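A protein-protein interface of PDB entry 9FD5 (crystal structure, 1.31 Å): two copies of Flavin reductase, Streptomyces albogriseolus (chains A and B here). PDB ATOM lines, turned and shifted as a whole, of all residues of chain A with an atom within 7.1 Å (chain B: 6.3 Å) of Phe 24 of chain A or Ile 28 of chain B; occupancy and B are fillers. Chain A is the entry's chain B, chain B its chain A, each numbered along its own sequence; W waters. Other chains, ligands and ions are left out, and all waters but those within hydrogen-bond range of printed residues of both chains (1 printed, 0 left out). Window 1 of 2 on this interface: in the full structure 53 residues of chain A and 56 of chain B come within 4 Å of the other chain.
Water W1 lies within hydrogen-bond range of the side-chain hydroxyl (OG1) of Thr 49 of chain B (2.8 Å), the backbone carbonyl oxygen (O) of Val 48 of chain B (3.2 Å) and the backbone carbonyl oxygen (O) of Ser 46 of chain A (3.3 Å).
3 positions are printed for both chains.
Of the 12 printed residues of chain A, 5 touch a printed residue of chain B.
Printed residues of chain A that touch a printed residue of chain B: Leu 20, Met 21, Ala 23, Phe 24 and Pro 25.
Among the printed residues, 14 pairs touch across the chains.
The backbone NH (N) of Gly 27 of chain B is in hydrogen-bond range of the backbone carbonyl oxygen (O) of Pro 25 of chain A (2.9 Å).
Leu 20 of chain A touches Leu 82 of chain B (CD1 to CD1, 3.7 Å).
CZ of Phe 122 of chain B touches O of Ala 23 of chain A, at 3.4 Å.
Ala 23 of chain A touches Pro 155 of chain B.
Phe 24 of chain A touches Thr 26 of chain B (CZ to CB, 3.9 Å).
Phe 24 of chain A touches Gly 27 of chain B.
Phe 24 of chain A touches Ile 28 of chain B (CE1 to N, 3.7 Å).
Phe 24 of chain A touches Val 48 of chain B (CE2 to O, 3.4 Å).
Phe 24 of chain A touches Leu 82 of chain B.
Pro 25 of chain A touches Pro 155 of chain B (CD to CB, 3.8 Å).
Pro 25 of chain A touches Leu 157 of chain B.
Of the printed residues of chain B, Phe 24 of chain A touches Thr 26 (3.9 Å), Gly 27 (3.3 Å), Ile 28 (3.7 Å), Ser 46 (3.7 Å), Val 48 (3.4 Å) and Leu 82 (3.9 Å).
Printed residues of chain A within 4 Å of Pro 155 of chain B: Ala 23 and Pro 25.
Printed residues of chain A within 4 Å of Thr 49 of chain B: Met 21 (3.8 Å).
The backbone NH of Tyr 158 of chain B is in hydrogen-bond range of the backbone carbonyl oxygen of Thr 26 of chain B.
The backbone carbonyl oxygen of Ile 28 of chain B sits at hydrogen-bond distance from the backbone NH of Leu 83 of chain B (3.0 Å).
O of Leu 82 of chain B lies within hydrogen-bond range of N of Phe 122 of chain B (2.9 Å).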
ATOM      1  N   ASP A  19      15.836 -19.482  24.660  1.00  0.00           N
ATOM      2  CA  ASP A  19      15.387 -18.543  23.634  1.00  0.00           C
ATOM      3  C   ASP A  19      16.536 -17.628  23.200  1.00  0.00           C
ATOM      4  O   ASP A  19      16.654 -17.259  22.019  1.00  0.00           O
ATOM      5  CB  ASP A  19      14.206 -17.698  24.123  1.00  0.00           C
ATOM      6  CG  ASP A  19      12.918 -18.487  24.368  1.00  0.00           C
ATOM      7  OD1 ASP A  19      12.783 -19.617  23.912  1.00  0.00           O
ATOM      8  OD2 ASP A  19      12.015 -17.908  25.026  1.00  0.00           O
ATOM      9  N   LEU A  20      17.363 -17.201  24.155  1.00  0.00           N
ATOM     10  CA  LEU A  20      18.539 -16.389  23.858  1.00  0.00           C
ATOM     11  C   LEU A  20      19.516 -17.151  22.979  1.00  0.00           C
ATOM     12  O   LEU A  20      19.934 -16.675  21.924  1.00  0.00           O
ATOM     13  CB  LEU A  20      19.210 -15.976  25.180  1.00  0.00           C
ATOM     14  CG  LEU A  20      20.593 -15.342  25.062  1.00  0.00           C
ATOM     15  CD1 LEU A  20      20.465 -13.942  24.601  1.00  0.00           C
ATOM     16  CD2 LEU A  20      21.322 -15.455  26.404  1.00  0.00           C
ATOM     17  N   MET A  21      19.951 -18.312  23.447  1.00  0.00           N
ATOM     18  CA  MET A  21      20.986 -19.051  22.735  1.00  0.00           C
ATOM     19  C   MET A  21      20.522 -19.578  21.398  1.00  0.00           C
ATOM     20  O   MET A  21      21.351 -19.751  20.493  1.00  0.00           O
ATOM     21  CB  MET A  21      21.567 -20.161  23.606  1.00  0.00           C
ATOM     22  CG  MET A  21      22.179 -19.646  24.927  1.00  0.00           C
ATOM     23  SD  MET A  21      23.400 -18.329  24.777  1.00  0.00           S
ATOM     24  CE  MET A  21      24.761 -19.222  24.066  1.00  0.00           C
ATOM     25  N   SER A  22      19.229 -19.808  21.236  1.00  0.00           N
ATOM     26  CA  SER A  22      18.732 -20.200  19.928  1.00  0.00           C
ATOM     27  C   SER A  22      19.065 -19.146  18.877  1.00  0.00           C
ATOM     28  O   SER A  22      19.326 -19.477  17.714  1.00  0.00           O
ATOM     29  CB  SER A  22      17.233 -20.405  20.037  1.00  0.00           C
ATOM     30  OG  SER A  22      16.697 -20.772  18.800  1.00  0.00           O
ATOM     31  N   ALA A  23      19.117 -17.883  19.285  1.00  0.00           N
ATOM     32  CA  ALA A  23      19.332 -16.759  18.384  1.00  0.00           C
ATOM     33  C   ALA A  23      20.806 -16.452  18.153  1.00  0.00           C
ATOM     34  O   ALA A  23      21.124 -15.429  17.554  1.00  0.00           O
ATOM     35  CB  ALA A  23      18.573 -15.548  18.921  1.00  0.00           C
ATOM     36  N   PHE A  24      21.704 -17.353  18.565  1.00  0.00           N
ATOM     37  CA  PHE A  24      23.122 -17.305  18.239  1.00  0.00           C
ATOM     38  C   PHE A  24      23.397 -18.440  17.261  1.00  0.00           C
ATOM     39  O   PHE A  24      23.642 -19.591  17.671  1.00  0.00           O
ATOM     40  CB  PHE A  24      24.006 -17.424  19.485  1.00  0.00           C
ATOM     41  CG  PHE A  24      25.493 -17.163  19.210  1.00  0.00           C
ATOM     42  CD1 PHE A  24      26.003 -15.888  19.216  1.00  0.00           C
ATOM     43  CD2 PHE A  24      26.356 -18.203  18.937  1.00  0.00           C
ATOM     44  CE1 PHE A  24      27.365 -15.658  18.957  1.00  0.00           C
ATOM     45  CE2 PHE A  24      27.702 -17.979  18.689  1.00  0.00           C
ATOM     46  CZ  PHE A  24      28.194 -16.704  18.693  1.00  0.00           C
ATOM     47  N   PRO A  25      23.307 -18.195  15.961  1.00  0.00           N
ATOM     48  CA  PRO A  25      23.417 -19.304  15.021  1.00  0.00           C
ATOM     49  C   PRO A  25      24.861 -19.760  14.915  1.00  0.00           C
ATOM     50  O   PRO A  25      25.804 -19.022  15.226  1.00  0.00           O
ATOM     51  CB  PRO A  25      22.896 -18.719  13.710  1.00  0.00           C
ATOM     52  CG  PRO A  25      22.070 -17.531  14.095  1.00  0.00           C
ATOM     53  CD  PRO A  25      22.861 -16.970  15.286  1.00  0.00           C
ATOM     54  N   THR A  26      25.019 -20.993  14.442  1.00  0.00           N
ATOM     55  CA  THR A  26      26.328 -21.598  14.291  1.00  0.00           C
ATOM     56  C   THR A  26      26.350 -22.562  13.114  1.00  0.00           C
ATOM     57  O   THR A  26      25.325 -22.973  12.587  1.00  0.00           O
ATOM     58  CB  THR A  26      26.719 -22.385  15.560  1.00  0.00           C
ATOM     59  OG1 THR A  26      25.845 -23.494  15.721  1.00  0.00           O
ATOM     60  CG2 THR A  26      26.715 -21.549  16.826  1.00  0.00           C
ATOM     61  N   SER A  46      27.001 -28.275  18.272  1.00  0.00           N
ATOM     62  CA  SER A  46      27.080 -26.889  17.817  1.00  0.00           C
ATOM     63  C   SER A  46      27.918 -26.022  18.750  1.00  0.00           C
ATOM     64  O   SER A  46      28.058 -24.817  18.509  1.00  0.00           O
ATOM     65  CB  SER A  46      25.695 -26.285  17.628  1.00  0.00           C
ATOM     66  OG  SER A  46      25.021 -26.316  18.876  1.00  0.00           O
ATOM     67  N   TYR A 158      22.721 -23.871  11.829  1.00  0.00           N
ATOM     68  CA  TYR A 158      21.580 -24.097  12.692  1.00  0.00           C
ATOM     69  C   TYR A 158      21.370 -22.836  13.513  1.00  0.00           C
ATOM     70  O   TYR A 158      22.308 -22.300  14.102  1.00  0.00           O
ATOM     71  CB  TYR A 158      21.758 -25.340  13.616  1.00  0.00           C
ATOM     72  CG  TYR A 158      20.458 -25.797  14.254  1.00  0.00           C
ATOM     73  CD1 TYR A 158      19.592 -26.623  13.568  1.00  0.00           C
ATOM     74  CD2 TYR A 158      20.079 -25.340  15.505  1.00  0.00           C
ATOM     75  CE1 TYR A 158      18.440 -27.050  14.137  1.00  0.00           C
ATOM     76  CE2 TYR A 158      18.909 -25.743  16.091  1.00  0.00           C
ATOM     77  CZ  TYR A 158      18.080 -26.594  15.393  1.00  0.00           C
ATOM     78  OH  TYR A 158      16.878 -26.991  15.943  1.00  0.00           O
ATOM     79  N   GLY A 159      20.130 -22.370  13.566  1.00  0.00           N
ATOM     80  CA  GLY A 159      19.827 -21.152  14.290  1.00  0.00           C
ATOM     81  C   GLY A 159      18.322 -20.961  14.311  1.00  0.00           C
ATOM     82  O   GLY A 159      17.633 -21.434  13.410  1.00  0.00           O
ATOM     83  N   LEU A 160      17.801 -20.299  15.336  1.00  0.00           N
ATOM     84  CA  LEU A 160      16.370 -20.035  15.401  1.00  0.00           C
ATOM     85  C   LEU A 160      15.597 -21.332  15.157  1.00  0.00           C
ATOM     86  O   LEU A 160      14.591 -21.379  14.440  1.00  0.00           O
ATOM     87  CB  LEU A 160      15.971 -18.910  14.437  1.00  0.00           C
ATOM     88  CG  LEU A 160      16.608 -17.549  14.764  1.00  0.00           C
ATOM     89  CD1 LEU A 160      16.274 -16.480  13.701  1.00  0.00           C
ATOM     90  CD2 LEU A 160      16.226 -17.067  16.177  1.00  0.00           C
ATOM     91  N   THR B  26      29.347 -18.202  12.874  1.00  0.00           N
ATOM     92  CA  THR B  26      28.732 -17.952  14.177  1.00  0.00           C
ATOM     93  C   THR B  26      27.959 -16.639  14.141  1.00  0.00           C
ATOM     94  O   THR B  26      28.141 -15.816  13.269  1.00  0.00           O
ATOM     95  CB  THR B  26      29.785 -17.842  15.301  1.00  0.00           C
ATOM     96  OG1 THR B  26      30.581 -16.681  15.088  1.00  0.00           O
ATOM     97  CG2 THR B  26      30.673 -19.055  15.373  1.00  0.00           C
ATOM     98  N   GLY B  27      27.168 -16.417  15.170  1.00  0.00           N
ATOM     99  CA  GLY B  27      26.703 -15.100  15.520  1.00  0.00           C
ATOM    100  C   GLY B  27      27.876 -14.252  15.988  1.00  0.00           C
ATOM    101  O   GLY B  27      29.036 -14.680  16.056  1.00  0.00           O
ATOM    102  N   ILE B  28      27.559 -13.005  16.324  1.00  0.00           N
ATOM    103  CA  ILE B  28      28.566 -12.033  16.730  1.00  0.00           C
ATOM    104  C   ILE B  28      28.031 -11.274  17.924  1.00  0.00           C
ATOM    105  O   ILE B  28      26.943 -10.699  17.857  1.00  0.00           O
ATOM    106  CB  ILE B  28      28.894 -11.024  15.616  1.00  0.00           C
ATOM    107  CG1 ILE B  28      29.774 -11.673  14.573  1.00  0.00           C
ATOM    108  CG2 ILE B  28      29.606  -9.801  16.227  1.00  0.00           C
ATOM    109  CD1 ILE B  28      31.243 -11.911  14.999  1.00  0.00           C
ATOM    110  N   ALA B  29      28.813 -11.229  18.989  1.00  0.00           N
ATOM    111  CA  ALA B  29      28.464 -10.472  20.158  1.00  0.00           C
ATOM    112  C   ALA B  29      29.447  -9.333  20.352  1.00  0.00           C
ATOM    113  O   ALA B  29      30.581  -9.352  19.852  1.00  0.00           O
ATOM    114  CB  ALA B  29      28.518 -11.377  21.374  1.00  0.00           C
ATOM    115  N   VAL B  30      29.018  -8.336  21.121  1.00  0.00           N
ATOM    116  CA  VAL B  30      29.940  -7.436  21.793  1.00  0.00           C
ATOM    117  C   VAL B  30      29.810  -7.725  23.282  1.00  0.00           C
ATOM    118  O   VAL B  30      28.704  -7.686  23.847  1.00  0.00           O
ATOM    119  CB  VAL B  30      29.677  -5.968  21.452  1.00  0.00           C
ATOM    120  CG1 VAL B  30      30.538  -5.046  22.268  1.00  0.00           C
ATOM    121  CG2 VAL B  30      29.842  -5.712  19.982  1.00  0.00           C
ATOM    122  N   THR B  44      34.430  -7.073  20.377  1.00  0.00           N
ATOM    123  CA  THR B  44      33.721  -8.014  19.530  1.00  0.00           C
ATOM    124  C   THR B  44      34.183  -9.424  19.830  1.00  0.00           C
ATOM    125  O   THR B  44      35.380  -9.679  19.969  1.00  0.00           O
ATOM    126  CB  THR B  44      34.002  -7.640  18.088  1.00  0.00           C
ATOM    127  OG1 THR B  44      33.543  -6.298  17.915  1.00  0.00           O
ATOM    128  CG2 THR B  44      33.350  -8.537  17.106  1.00  0.00           C
ATOM    129  N   CYS B  45      33.226 -10.348  19.912  1.00  0.00           N
ATOM    130  CA  CYS B  45      33.491 -11.717  20.345  1.00  0.00           C
ATOM    131  C   CYS B  45      32.609 -12.681  19.564  1.00  0.00           C
ATOM    132  O   CYS B  45      31.378 -12.589  19.622  1.00  0.00           O
ATOM    133  CB  CYS B  45      33.219 -11.824  21.849  1.00  0.00           C
ATOM    134  SG  CYS B  45      33.304 -13.447  22.560  1.00  0.00           S
ATOM    135  N   SER B  46      33.238 -13.635  18.862  1.00  0.00           N
ATOM    136  CA  SER B  46      32.524 -14.701  18.192  1.00  0.00           C
ATOM    137  C   SER B  46      32.582 -16.015  18.960  1.00  0.00           C
ATOM    138  O   SER B  46      31.850 -16.935  18.617  1.00  0.00           O
ATOM    139  CB  SER B  46      33.085 -14.897  16.785  1.00  0.00           C
ATOM    140  OG  SER B  46      34.477 -15.118  16.765  1.00  0.00           O
ATOM    141  N   SER B  47      33.483 -16.156  19.922  1.00  0.00           N
ATOM    142  CA  SER B  47      33.603 -17.395  20.677  1.00  0.00           C
ATOM    143  C   SER B  47      32.707 -17.273  21.904  1.00  0.00           C
ATOM    144  O   SER B  47      33.169 -16.916  22.999  1.00  0.00           O
ATOM    145  CB  SER B  47      35.061 -17.660  21.044  1.00  0.00           C
ATOM    146  OG  SER B  47      35.841 -18.012  19.893  1.00  0.00           O
ATOM    147  N   VAL B  48      31.390 -17.470  21.668  1.00  0.00           N
ATOM    148  CA  VAL B  48      30.317 -17.566  22.654  1.00  0.00           C
ATOM    149  C   VAL B  48      29.654 -18.915  22.460  1.00  0.00           C
ATOM    150  O   VAL B  48      29.380 -19.313  21.322  1.00  0.00           O
ATOM    151  CB  VAL B  48      29.250 -16.497  22.372  1.00  0.00           C
ATOM    152  CG1 VAL B  48      28.154 -16.552  23.433  1.00  0.00           C
ATOM    153  CG2 VAL B  48      29.859 -15.109  22.258  1.00  0.00           C
ATOM    154  N   THR B  49      29.457 -19.669  23.541  1.00  0.00           N
ATOM    155  CA  THR B  49      28.667 -20.884  23.434  1.00  0.00           C
ATOM    156  C   THR B  49      27.982 -21.191  24.747  1.00  0.00           C
ATOM    157  O   THR B  49      28.280 -20.610  25.778  1.00  0.00           O
ATOM    158  CB  THR B  49      29.438 -22.114  22.894  1.00  0.00           C
ATOM    159  OG1 THR B  49      28.503 -23.124  22.488  1.00  0.00           O
ATOM    160  CG2 THR B  49      30.285 -22.757  23.917  1.00  0.00           C
ATOM    161  N   ASN B  81      26.101  -8.883  24.270  1.00  0.00           N
ATOM    162  CA  ASN B  81      25.171  -8.162  23.416  1.00  0.00           C
ATOM    163  C   ASN B  81      25.172  -8.862  22.059  1.00  0.00           C
ATOM    164  O   ASN B  81      26.162  -8.785  21.322  1.00  0.00           O
ATOM    165  CB  ASN B  81      25.649  -6.729  23.221  1.00  0.00           C
ATOM    166  CG  ASN B  81      25.559  -5.882  24.459  1.00  0.00           C
ATOM    167  OD1 ASN B  81      24.608  -5.149  24.666  1.00  0.00           O
ATOM    168  ND2 ASN B  81      26.595  -5.959  25.288  1.00  0.00           N
ATOM    169  N   LEU B  82      24.090  -9.560  21.732  1.00  0.00           N
ATOM    170  CA  LEU B  82      24.011 -10.275  20.467  1.00  0.00           C
ATOM    171  C   LEU B  82      23.579  -9.309  19.365  1.00  0.00           C
ATOM    172  O   LEU B  82      22.482  -8.738  19.421  1.00  0.00           O
ATOM    173  CB  LEU B  82      23.026 -11.439  20.578  1.00  0.00           C
ATOM    174  CG  LEU B  82      23.372 -12.534  21.568  1.00  0.00           C
ATOM    175  CD1 LEU B  82      22.360 -13.660  21.422  1.00  0.00           C
ATOM    176  CD2 LEU B  82      24.796 -13.000  21.469  1.00  0.00           C
ATOM    177  N   LEU B  83      24.401  -9.177  18.332  1.00  0.00           N
ATOM    178  CA  LEU B  83      24.171  -8.187  17.290  1.00  0.00           C
ATOM    179  C   LEU B  83      23.182  -8.664  16.246  1.00  0.00           C
ATOM    180  O   LEU B  83      23.233  -9.812  15.790  1.00  0.00           O
ATOM    181  CB  LEU B  83      25.481  -7.834  16.627  1.00  0.00           C
ATOM    182  CG  LEU B  83      26.581  -7.249  17.513  1.00  0.00           C
ATOM    183  CD1 LEU B  83      27.777  -6.895  16.630  1.00  0.00           C
ATOM    184  CD2 LEU B  83      26.088  -6.048  18.284  1.00  0.00           C
ATOM    185  N   HIS B  84      22.290  -7.749  15.858  1.00  0.00           N
ATOM    186  CA  HIS B  84      21.423  -7.980  14.722  1.00  0.00           C
ATOM    187  C   HIS B  84      22.091  -7.557  13.423  1.00  0.00           C
ATOM    188  O   HIS B  84      23.203  -7.034  13.404  1.00  0.00           O
ATOM    189  CB  HIS B  84      20.056  -7.324  14.909  1.00  0.00           C
ATOM    190  CG  HIS B  84      20.098  -5.860  15.124  1.00  0.00           C
ATOM    191  ND1 HIS B  84      20.606  -4.983  14.197  1.00  0.00           N
ATOM    192  CD2 HIS B  84      19.660  -5.115  16.161  1.00  0.00           C
ATOM    193  CE1 HIS B  84      20.484  -3.750  14.658  1.00  0.00           C
ATOM    194  NE2 HIS B  84      19.918  -3.802  15.851  1.00  0.00           N
ATOM    195  N   GLY B  87      24.027  -4.393  12.883  1.00  0.00           N
ATOM    196  CA  GLY B  87      25.082  -4.121  13.825  1.00  0.00           C
ATOM    197  C   GLY B  87      26.495  -4.318  13.329  1.00  0.00           C
ATOM    198  O   GLY B  87      27.417  -4.349  14.133  1.00  0.00           O
ATOM    199  N   ALA B  91      30.280  -4.121  15.368  1.00  0.00           N
ATOM    200  CA  ALA B  91      31.290  -5.177  15.405  1.00  0.00           C
ATOM    201  C   ALA B  91      32.649  -4.664  14.935  1.00  0.00           C
ATOM    202  O   ALA B  91      33.692  -5.087  15.440  1.00  0.00           O
ATOM    203  CB  ALA B  91      30.814  -6.359  14.567  1.00  0.00           C
ATOM    204  N   PHE B 122      20.014  -7.216  19.386  1.00  0.00           N
ATOM    205  CA  PHE B 122      18.649  -7.644  19.617  1.00  0.00           C
ATOM    206  C   PHE B 122      18.447  -8.351  20.956  1.00  0.00           C
ATOM    207  O   PHE B 122      17.300  -8.558  21.369  1.00  0.00           O
ATOM    208  CB  PHE B 122      18.146  -8.532  18.467  1.00  0.00           C
ATOM    209  CG  PHE B 122      18.808  -9.870  18.408  1.00  0.00           C
ATOM    210  CD1 PHE B 122      18.300 -10.931  19.151  1.00  0.00           C
ATOM    211  CD2 PHE B 122      19.978 -10.056  17.688  1.00  0.00           C
ATOM    212  CE1 PHE B 122      18.925 -12.147  19.139  1.00  0.00           C
ATOM    213  CE2 PHE B 122      20.614 -11.284  17.683  1.00  0.00           C
ATOM    214  CZ  PHE B 122      20.088 -12.323  18.421  1.00  0.00           C
ATOM    215  N   PRO B 155      19.761 -12.207  13.377  1.00  0.00           N
ATOM    216  CA  PRO B 155      21.153 -12.203  13.836  1.00  0.00           C
ATOM    217  C   PRO B 155      22.148 -11.875  12.729  1.00  0.00           C
ATOM    218  O   PRO B 155      22.054 -12.352  11.599  1.00  0.00           O
ATOM    219  CB  PRO B 155      21.357 -13.627  14.360  1.00  0.00           C
ATOM    220  CG  PRO B 155      20.018 -14.114  14.678  1.00  0.00           C
ATOM    221  CD  PRO B 155      19.083 -13.477  13.687  1.00  0.00           C
ATOM    222  N   LEU B 156      23.134 -11.074  13.096  1.00  0.00           N
ATOM    223  CA  LEU B 156      24.337 -10.919  12.286  1.00  0.00           C
ATOM    224  C   LEU B 156      25.159 -12.193  12.376  1.00  0.00           C
ATOM    225  O   LEU B 156      25.229 -12.813  13.425  1.00  0.00           O
ATOM    226  CB  LEU B 156      25.144  -9.740  12.830  1.00  0.00           C
ATOM    227  CG  LEU B 156      26.347  -9.274  12.027  1.00  0.00           C
ATOM    228  CD1 LEU B 156      25.874  -8.753  10.673  1.00  0.00           C
ATOM    229  CD2 LEU B 156      27.096  -8.169  12.789  1.00  0.00           C
ATOM    230  N   LEU B 157      25.828 -12.565  11.288  1.00  0.00           N
ATOM    231  CA  LEU B 157      26.720 -13.709  11.268  1.00  0.00           C
ATOM    232  C   LEU B 157      28.102 -13.265  10.821  1.00  0.00           C
ATOM    233  O   LEU B 157      28.275 -12.275  10.098  1.00  0.00           O
ATOM    234  CB  LEU B 157      26.262 -14.806  10.300  1.00  0.00           C
ATOM    235  CG  LEU B 157      24.843 -15.331  10.445  1.00  0.00           C
ATOM    236  CD1 LEU B 157      24.562 -16.311   9.329  1.00  0.00           C
ATOM    237  CD2 LEU B 157      24.652 -15.971  11.806  1.00  0.00           C
ATOM    238  N   TYR B 158      29.073 -14.060  11.218  1.00  0.00           N
ATOM    239  CA  TYR B 158      30.431 -13.955  10.731  1.00  0.00           C
ATOM    240  C   TYR B 158      30.887 -15.344  10.327  1.00  0.00           C
ATOM    241  O   TYR B 158      30.757 -16.293  11.100  1.00  0.00           O
ATOM    242  CB  TYR B 158      31.414 -13.345  11.756  1.00  0.00           C
ATOM    243  CG  TYR B 158      32.687 -12.838  11.108  1.00  0.00           C
ATOM    244  CD1 TYR B 158      32.748 -11.594  10.507  1.00  0.00           C
ATOM    245  CD2 TYR B 158      33.815 -13.605  11.100  1.00  0.00           C
ATOM    246  CE1 TYR B 158      33.912 -11.133   9.893  1.00  0.00           C
ATOM    247  CE2 TYR B 158      34.988 -13.168  10.492  1.00  0.00           C
ATOM    248  CZ  TYR B 158      35.036 -11.924   9.896  1.00  0.00           C
ATOM    249  OH  TYR B 158      36.196 -11.467   9.299  1.00  0.00           O
ATOM    250  N   PHE B 163      31.136 -10.815   6.979  1.00  0.00           N
ATOM    251  CA  PHE B 163      29.859 -10.649   7.631  1.00  0.00           C
ATOM    252  C   PHE B 163      28.738 -11.094   6.703  1.00  0.00           C
ATOM    253  O   PHE B 163      28.799 -10.923   5.488  1.00  0.00           O
ATOM    254  CB  PHE B 163      29.613  -9.172   7.981  1.00  0.00           C
ATOM    255  CG  PHE B 163      30.481  -8.658   9.090  1.00  0.00           C
ATOM    256  CD1 PHE B 163      30.160  -8.875  10.409  1.00  0.00           C
ATOM    257  CD2 PHE B 163      31.662  -8.011   8.816  1.00  0.00           C
ATOM    258  CE1 PHE B 163      30.964  -8.394  11.431  1.00  0.00           C
ATOM    259  CE2 PHE B 163      32.489  -7.531   9.858  1.00  0.00           C
ATOM    260  CZ  PHE B 163      32.126  -7.748  11.165  1.00  0.00           C
HETATM  261  O   HOH W   1      28.045 -21.916  19.998  1.00  0.00           O
